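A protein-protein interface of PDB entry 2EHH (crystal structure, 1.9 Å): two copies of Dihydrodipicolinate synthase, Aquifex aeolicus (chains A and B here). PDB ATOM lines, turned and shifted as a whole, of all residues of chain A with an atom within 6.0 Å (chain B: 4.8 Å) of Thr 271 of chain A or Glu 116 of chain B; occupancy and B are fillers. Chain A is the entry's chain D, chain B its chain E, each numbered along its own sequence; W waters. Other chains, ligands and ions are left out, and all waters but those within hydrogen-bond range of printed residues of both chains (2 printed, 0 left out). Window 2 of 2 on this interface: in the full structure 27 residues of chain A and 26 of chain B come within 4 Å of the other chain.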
ATOM      1  N   GLU A 246      33.289  -4.718 -31.900  1.00  0.00           N
ATOM      2  CA  GLU A 246      32.426  -5.826 -31.518  1.00  0.00           C
ATOM      3  C   GLU A 246      31.591  -5.303 -30.353  1.00  0.00           C
ATOM      4  O   GLU A 246      31.938  -4.289 -29.746  1.00  0.00           O
ATOM      5  CB  GLU A 246      33.238  -7.066 -31.117  1.00  0.00           C
ATOM      6  CG  GLU A 246      33.739  -7.870 -32.315  1.00  0.00           C
ATOM      7  CD  GLU A 246      34.350  -9.210 -31.933  1.00  0.00           C
ATOM      8  OE1 GLU A 246      33.939  -9.788 -30.900  1.00  0.00           O
ATOM      9  OE2 GLU A 246      35.227  -9.698 -32.679  1.00  0.00           O
ATOM     10  N   ILE A 250      32.844  -6.259 -24.999  1.00  0.00           N
ATOM     11  CA  ILE A 250      33.851  -7.230 -25.417  1.00  0.00           C
ATOM     12  C   ILE A 250      35.198  -6.555 -25.742  1.00  0.00           C
ATOM     13  O   ILE A 250      36.246  -6.971 -25.242  1.00  0.00           O
ATOM     14  CB  ILE A 250      33.345  -8.101 -26.600  1.00  0.00           C
ATOM     15  CG1 ILE A 250      32.200  -9.002 -26.112  1.00  0.00           C
ATOM     16  CG2 ILE A 250      34.480  -8.974 -27.131  1.00  0.00           C
ATOM     17  CD1 ILE A 250      31.572  -9.906 -27.177  1.00  0.00           C
ATOM     18  N   PHE A 266      34.957 -13.529 -19.793  1.00  0.00           N
ATOM     19  CA  PHE A 266      33.608 -12.996 -19.938  1.00  0.00           C
ATOM     20  C   PHE A 266      32.638 -14.061 -19.455  1.00  0.00           C
ATOM     21  O   PHE A 266      33.034 -15.186 -19.156  1.00  0.00           O
ATOM     22  CB  PHE A 266      33.276 -12.710 -21.408  1.00  0.00           C
ATOM     23  CG  PHE A 266      34.158 -11.685 -22.049  1.00  0.00           C
ATOM     24  CD1 PHE A 266      35.359 -12.056 -22.647  1.00  0.00           C
ATOM     25  CD2 PHE A 266      33.783 -10.346 -22.072  1.00  0.00           C
ATOM     26  CE1 PHE A 266      36.173 -11.102 -23.264  1.00  0.00           C
ATOM     27  CE2 PHE A 266      34.588  -9.391 -22.683  1.00  0.00           C
ATOM     28  CZ  PHE A 266      35.785  -9.770 -23.280  1.00  0.00           C
ATOM     29  N   ARG A 267      31.365 -13.700 -19.369  1.00  0.00           N
ATOM     30  CA  ARG A 267      30.343 -14.663 -18.996  1.00  0.00           C
ATOM     31  C   ARG A 267      29.438 -14.796 -20.203  1.00  0.00           C
ATOM     32  O   ARG A 267      28.959 -13.786 -20.719  1.00  0.00           O
ATOM     33  CB  ARG A 267      29.528 -14.189 -17.796  1.00  0.00           C
ATOM     34  CG  ARG A 267      30.239 -14.400 -16.472  1.00  0.00           C
ATOM     35  CD  ARG A 267      29.318 -14.137 -15.305  1.00  0.00           C
ATOM     36  NE  ARG A 267      29.989 -14.401 -14.038  1.00  0.00           N
ATOM     37  CZ  ARG A 267      29.452 -14.159 -12.851  1.00  0.00           C
ATOM     38  NH1 ARG A 267      28.233 -13.646 -12.773  1.00  0.00           N
ATOM     39  NH2 ARG A 267      30.136 -14.428 -11.745  1.00  0.00           N
ATOM     40  N   LEU A 268      29.228 -16.030 -20.660  1.00  0.00           N
ATOM     41  CA  LEU A 268      28.363 -16.290 -21.805  1.00  0.00           C
ATOM     42  C   LEU A 268      26.999 -15.667 -21.526  1.00  0.00           C
ATOM     43  O   LEU A 268      26.533 -15.675 -20.389  1.00  0.00           O
ATOM     44  CB  LEU A 268      28.207 -17.801 -22.030  1.00  0.00           C
ATOM     45  CG  LEU A 268      29.418 -18.552 -22.599  1.00  0.00           C
ATOM     46  CD1 LEU A 268      29.160 -20.052 -22.586  1.00  0.00           C
ATOM     47  CD2 LEU A 268      29.695 -18.081 -24.017  1.00  0.00           C
ATOM     48  N   PRO A 269      26.297 -15.208 -22.572  1.00  0.00           N
ATOM     49  CA  PRO A 269      26.652 -15.236 -23.994  1.00  0.00           C
ATOM     50  C   PRO A 269      27.771 -14.335 -24.531  1.00  0.00           C
ATOM     51  O   PRO A 269      28.010 -14.324 -25.738  1.00  0.00           O
ATOM     52  CB  PRO A 269      25.311 -14.966 -24.676  1.00  0.00           C
ATOM     53  CG  PRO A 269      24.675 -13.985 -23.751  1.00  0.00           C
ATOM     54  CD  PRO A 269      24.972 -14.586 -22.375  1.00  0.00           C
ATOM     55  N   LEU A 270      28.455 -13.574 -23.678  1.00  0.00           N
ATOM     56  CA  LEU A 270      29.546 -12.747 -24.195  1.00  0.00           C
ATOM     57  C   LEU A 270      30.762 -13.654 -24.350  1.00  0.00           C
ATOM     58  O   LEU A 270      30.952 -14.582 -23.565  1.00  0.00           O
ATOM     59  CB  LEU A 270      29.856 -11.566 -23.266  1.00  0.00           C
ATOM     60  CG  LEU A 270      28.782 -10.468 -23.218  1.00  0.00           C
ATOM     61  CD1 LEU A 270      29.392  -9.201 -22.626  1.00  0.00           C
ATOM     62  CD2 LEU A 270      28.252 -10.170 -24.629  1.00  0.00           C
ATOM     63  N   THR A 271      31.575 -13.387 -25.369  1.00  0.00           N
ATOM     64  CA  THR A 271      32.748 -14.207 -25.665  1.00  0.00           C
ATOM     65  C   THR A 271      33.948 -13.338 -26.013  1.00  0.00           C
ATOM     66  O   THR A 271      33.818 -12.125 -26.167  1.00  0.00           O
ATOM     67  CB  THR A 271      32.479 -15.100 -26.889  1.00  0.00           C
ATOM     68  OG1 THR A 271      32.107 -14.266 -27.997  1.00  0.00           O
ATOM     69  CG2 THR A 271      31.335 -16.082 -26.611  1.00  0.00           C
ATOM     70  N   GLU A 272      35.114 -13.967 -26.147  1.00  0.00           N
ATOM     71  CA  GLU A 272      36.321 -13.244 -26.522  1.00  0.00           C
ATOM     72  C   GLU A 272      36.129 -12.802 -27.974  1.00  0.00           C
ATOM     73  O   GLU A 272      35.321 -13.387 -28.702  1.00  0.00           O
ATOM     74  CB  GLU A 272      37.551 -14.152 -26.405  1.00  0.00           C
ATOM     75  CG  GLU A 272      37.667 -14.874 -25.073  1.00  0.00           C
ATOM     76  CD  GLU A 272      39.005 -15.577 -24.893  1.00  0.00           C
ATOM     77  OE1 GLU A 272      39.585 -16.042 -25.897  1.00  0.00           O
ATOM     78  OE2 GLU A 272      39.472 -15.674 -23.741  1.00  0.00           O
ATOM     79  N   MET A 273      36.865 -11.774 -28.388  1.00  0.00           N
ATOM     80  CA  MET A 273      36.778 -11.228 -29.742  1.00  0.00           C
ATOM     81  C   MET A 273      37.219 -12.209 -30.822  1.00  0.00           C
ATOM     82  O   MET A 273      37.883 -13.203 -30.532  1.00  0.00           O
ATOM     83  CB  MET A 273      37.664  -9.988 -29.858  1.00  0.00           C
ATOM     84  CG  MET A 273      37.365  -8.896 -28.859  1.00  0.00           C
ATOM     85  SD  MET A 273      38.615  -7.605 -28.925  1.00  0.00           S
ATOM     86  CE  MET A 273      38.107  -6.735 -30.439  1.00  0.00           C
ATOM     87  N   THR B 110      27.757 -11.588 -29.984  1.00  0.00           N
ATOM     88  CA  THR B 110      28.213 -11.771 -31.355  1.00  0.00           C
ATOM     89  C   THR B 110      27.639 -13.110 -31.817  1.00  0.00           C
ATOM     90  O   THR B 110      27.099 -13.861 -31.005  1.00  0.00           O
ATOM     91  CB  THR B 110      29.745 -11.840 -31.421  1.00  0.00           C
ATOM     92  OG1 THR B 110      30.196 -12.984 -30.686  1.00  0.00           O
ATOM     93  CG2 THR B 110      30.368 -10.584 -30.812  1.00  0.00           C
ATOM     94  N   ARG B 112      29.207 -15.701 -32.600  1.00  0.00           N
ATOM     95  CA  ARG B 112      29.932 -16.761 -31.908  1.00  0.00           C
ATOM     96  C   ARG B 112      29.315 -16.922 -30.525  1.00  0.00           C
ATOM     97  O   ARG B 112      29.181 -18.035 -30.018  1.00  0.00           O
ATOM     98  CB  ARG B 112      31.416 -16.417 -31.768  1.00  0.00           C
ATOM     99  CG  ARG B 112      32.220 -17.507 -31.070  1.00  0.00           C
ATOM    100  CD  ARG B 112      32.161 -18.810 -31.865  1.00  0.00           C
ATOM    101  NE  ARG B 112      32.817 -19.922 -31.182  1.00  0.00           N
ATOM    102  CZ  ARG B 112      32.942 -21.144 -31.695  1.00  0.00           C
ATOM    103  NH1 ARG B 112      32.455 -21.412 -32.901  1.00  0.00           N
ATOM    104  NH2 ARG B 112      33.549 -22.098 -31.002  1.00  0.00           N
ATOM    105  N   GLY B 113      28.937 -15.798 -29.923  1.00  0.00           N
ATOM    106  CA  GLY B 113      28.323 -15.836 -28.609  1.00  0.00           C
ATOM    107  C   GLY B 113      26.975 -16.531 -28.653  1.00  0.00           C
ATOM    108  O   GLY B 113      26.614 -17.251 -27.726  1.00  0.00           O
ATOM    109  N   LEU B 114      26.223 -16.315 -29.728  1.00  0.00           N
ATOM    110  CA  LEU B 114      24.916 -16.947 -29.867  1.00  0.00           C
ATOM    111  C   LEU B 114      25.106 -18.445 -30.080  1.00  0.00           C
ATOM    112  O   LEU B 114      24.336 -19.261 -29.573  1.00  0.00           O
ATOM    113  CB  LEU B 114      24.150 -16.338 -31.049  1.00  0.00           C
ATOM    114  CG  LEU B 114      23.817 -14.848 -30.916  1.00  0.00           C
ATOM    115  CD1 LEU B 114      23.075 -14.378 -32.160  1.00  0.00           C
ATOM    116  CD2 LEU B 114      22.963 -14.623 -29.673  1.00  0.00           C
ATOM    117  N   TYR B 115      26.135 -18.805 -30.838  1.00  0.00           N
ATOM    118  CA  TYR B 115      26.434 -20.208 -31.084  1.00  0.00           C
ATOM    119  C   TYR B 115      26.750 -20.904 -29.761  1.00  0.00           C
ATOM    120  O   TYR B 115      26.184 -21.953 -29.440  1.00  0.00           O
ATOM    121  CB  TYR B 115      27.637 -20.336 -32.023  1.00  0.00           C
ATOM    122  CG  TYR B 115      28.202 -21.739 -32.121  1.00  0.00           C
ATOM    123  CD1 TYR B 115      27.481 -22.764 -32.733  1.00  0.00           C
ATOM    124  CD2 TYR B 115      29.465 -22.036 -31.612  1.00  0.00           C
ATOM    125  CE1 TYR B 115      28.010 -24.054 -32.843  1.00  0.00           C
ATOM    126  CE2 TYR B 115      30.004 -23.323 -31.713  1.00  0.00           C
ATOM    127  CZ  TYR B 115      29.271 -24.322 -32.331  1.00  0.00           C
ATOM    128  OH  TYR B 115      29.809 -25.582 -32.449  1.00  0.00           O
ATOM    129  N   GLU B 116      27.653 -20.312 -28.988  1.00  0.00           N
ATOM    130  CA  GLU B 116      28.039 -20.905 -27.716  1.00  0.00           C
ATOM    131  C   GLU B 116      26.894 -20.933 -26.710  1.00  0.00           C
ATOM    132  O   GLU B 116      26.783 -21.864 -25.915  1.00  0.00           O
ATOM    133  CB  GLU B 116      29.227 -20.148 -27.138  1.00  0.00           C
ATOM    134  CG  GLU B 116      30.328 -19.937 -28.154  1.00  0.00           C
ATOM    135  CD  GLU B 116      31.672 -20.398 -27.661  1.00  0.00           C
ATOM    136  OE1 GLU B 116      31.836 -21.620 -27.459  1.00  0.00           O
ATOM    137  OE2 GLU B 116      32.563 -19.541 -27.476  1.00  0.00           O
ATOM    138  N   HIS B 117      26.044 -19.910 -26.742  1.00  0.00           N
ATOM    139  CA  HIS B 117      24.900 -19.848 -25.835  1.00  0.00           C
ATOM    140  C   HIS B 117      23.991 -21.059 -26.067  1.00  0.00           C
ATOM    141  O   HIS B 117      23.755 -21.857 -25.157  1.00  0.00           O
ATOM    142  CB  HIS B 117      24.113 -18.556 -26.081  1.00  0.00           C
ATOM    143  CG  HIS B 117      22.864 -18.436 -25.265  1.00  0.00           C
ATOM    144  ND1 HIS B 117      22.877 -18.167 -23.912  1.00  0.00           N
ATOM    145  CD2 HIS B 117      21.558 -18.523 -25.617  1.00  0.00           C
ATOM    146  CE1 HIS B 117      21.637 -18.091 -23.467  1.00  0.00           C
ATOM    147  NE2 HIS B 117      20.814 -18.302 -24.482  1.00  0.00           N
ATOM    148  N   PHE B 118      23.490 -21.197 -27.290  1.00  0.00           N
ATOM    149  CA  PHE B 118      22.602 -22.304 -27.636  1.00  0.00           C
ATOM    150  C   PHE B 118      23.261 -23.684 -27.583  1.00  0.00           C
ATOM    151  O   PHE B 118      22.629 -24.658 -27.174  1.00  0.00           O
ATOM    152  CB  PHE B 118      21.983 -22.057 -29.017  1.00  0.00           C
ATOM    153  CG  PHE B 118      20.896 -21.005 -29.011  1.00  0.00           C
ATOM    154  CD1 PHE B 118      19.619 -21.307 -28.540  1.00  0.00           C
ATOM    155  CD2 PHE B 118      21.157 -19.712 -29.447  1.00  0.00           C
ATOM    156  CE1 PHE B 118      18.613 -20.334 -28.504  1.00  0.00           C
ATOM    157  CE2 PHE B 118      20.159 -18.729 -29.415  1.00  0.00           C
ATOM    158  CZ  PHE B 118      18.885 -19.043 -28.941  1.00  0.00           C
ATOM    159  N   LYS B 119      24.521 -23.778 -27.995  1.00  0.00           N
ATOM    160  CA  LYS B 119      25.216 -25.060 -27.958  1.00  0.00           C
ATOM    161  C   LYS B 119      25.342 -25.534 -26.511  1.00  0.00           C
ATOM    162  O   LYS B 119      25.112 -26.701 -26.205  1.00  0.00           O
ATOM    163  CB  LYS B 119      26.612 -24.934 -28.575  1.00  0.00           C
ATOM    164  CG  LYS B 119      27.438 -26.222 -28.520  1.00  0.00           C
ATOM    165  CD  LYS B 119      28.815 -26.011 -29.143  1.00  0.00           C
ATOM    166  CE  LYS B 119      29.634 -27.292 -29.156  1.00  0.00           C
ATOM    167  NZ  LYS B 119      28.996 -28.351 -29.997  1.00  0.00           N
ATOM    168  N   THR B 120      25.702 -24.616 -25.621  1.00  0.00           N
ATOM    169  CA  THR B 120      25.856 -24.951 -24.210  1.00  0.00           C
ATOM    170  C   THR B 120      24.557 -25.481 -23.619  1.00  0.00           C
ATOM    171  O   THR B 120      24.545 -26.514 -22.944  1.00  0.00           O
ATOM    172  CB  THR B 120      26.314 -23.723 -23.396  1.00  0.00           C
ATOM    173  OG1 THR B 120      27.601 -23.297 -23.860  1.00  0.00           O
ATOM    174  CG2 THR B 120      26.412 -24.073 -21.925  1.00  0.00           C
HETATM  175  O   HOH W   1      29.274 -12.613 -27.602  1.00  0.00           O
HETATM  176  O   HOH W   2      33.248 -12.422 -30.445  1.00  0.00           O
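The side-chain hydroxyl (OG1) of Thr 110 of chain B lies within hydrogen-bond range of the backbone NH (N) of Gly 113 of chain B. The backbone carbonyl oxygen (O) of Glu 116 of chain B lies within hydrogen-bond range of the side-chain hydroxyl (OG1) of Thr 120 of chain B (2.6 Å). The guanidinium group (NE) of Arg 112 of chain B is in salt-bridge range of the side-chain carboxylate (OE2) of Glu 116 of chain B. N of Arg 112 of chain B sits close to OG1 of Thr 110 of chain B, 3.5 Å away.
Among the printed residues, merely in contact across the chains: Glu 246 of chain A with Thr 110 of chain B, Ile 250 of chain A with Thr 110 of chain B, Leu 268 of chain A with Glu 116 of chain B, Leu 268 of chain A with Thr 120 of chain B, Pro 269 of chain A with Gly 113 of chain B, Thr 271 of chain A with Thr 110 of chain B, Thr 271 of chain A with Gly 113 of chain B and Thr 271 of chain A with Glu 116 of chain B.
Of the printed residues of chain B, Glu 246 of chain A touches Thr 110 (3.7 Å). Of the printed residues of chain B, Leu 268 of chain A touches Glu 116 (3.8 Å) and Thr 120 (3.8 Å). Printed residues of chain B within 4 Å of Pro 269 of chain A: Gly 113. Leu 270 of chain A touches none of the printed residues of chain B. Of the printed residues of chain B, Thr 271 of chain A touches Thr 110, Gly 113 and Glu 116. Of the printed residues of chain A, Gly 113 of chain B touches Pro 269 (3.3 Å) and Thr 271 (3.6 Å). Glu 116 of chain B touches just these residues of chain A: Leu 268 (3.8 Å) and Thr 271 (3.8 Å). Of the printed residues of chain A, Thr 120 of chain B touches Leu 268 (3.8 Å). The nearest residue of chain B that does not touch Thr 271 of chain A is Arg 112 of chain B (4.4 Å).
Among the printed residues, 8 pairs touch across the chains.
No position is printed for both chains. Of the 8 pairs that touch across the chains among the printed residues, none has its exchanged pair printed and touching as well.
Water W2 lies within hydrogen-bond range of the side-chain carboxylate of Glu 246 of chain A (2.8 Å), the backbone carbonyl oxygen of Glu 272 of chain A (2.9 Å), the side-chain hydroxyl of Thr 110 of chain B (3.1 Å) and the side-chain hydroxyl of Thr 271 of chain A (3.3 Å). Water W1 lies within hydrogen-bond range of the backbone carbonyl oxygen (O) of Pro 269 of chain A, the backbone NH (N) of Thr 110 of chain B and the backbone NH (N) of Thr 271 of chain A.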
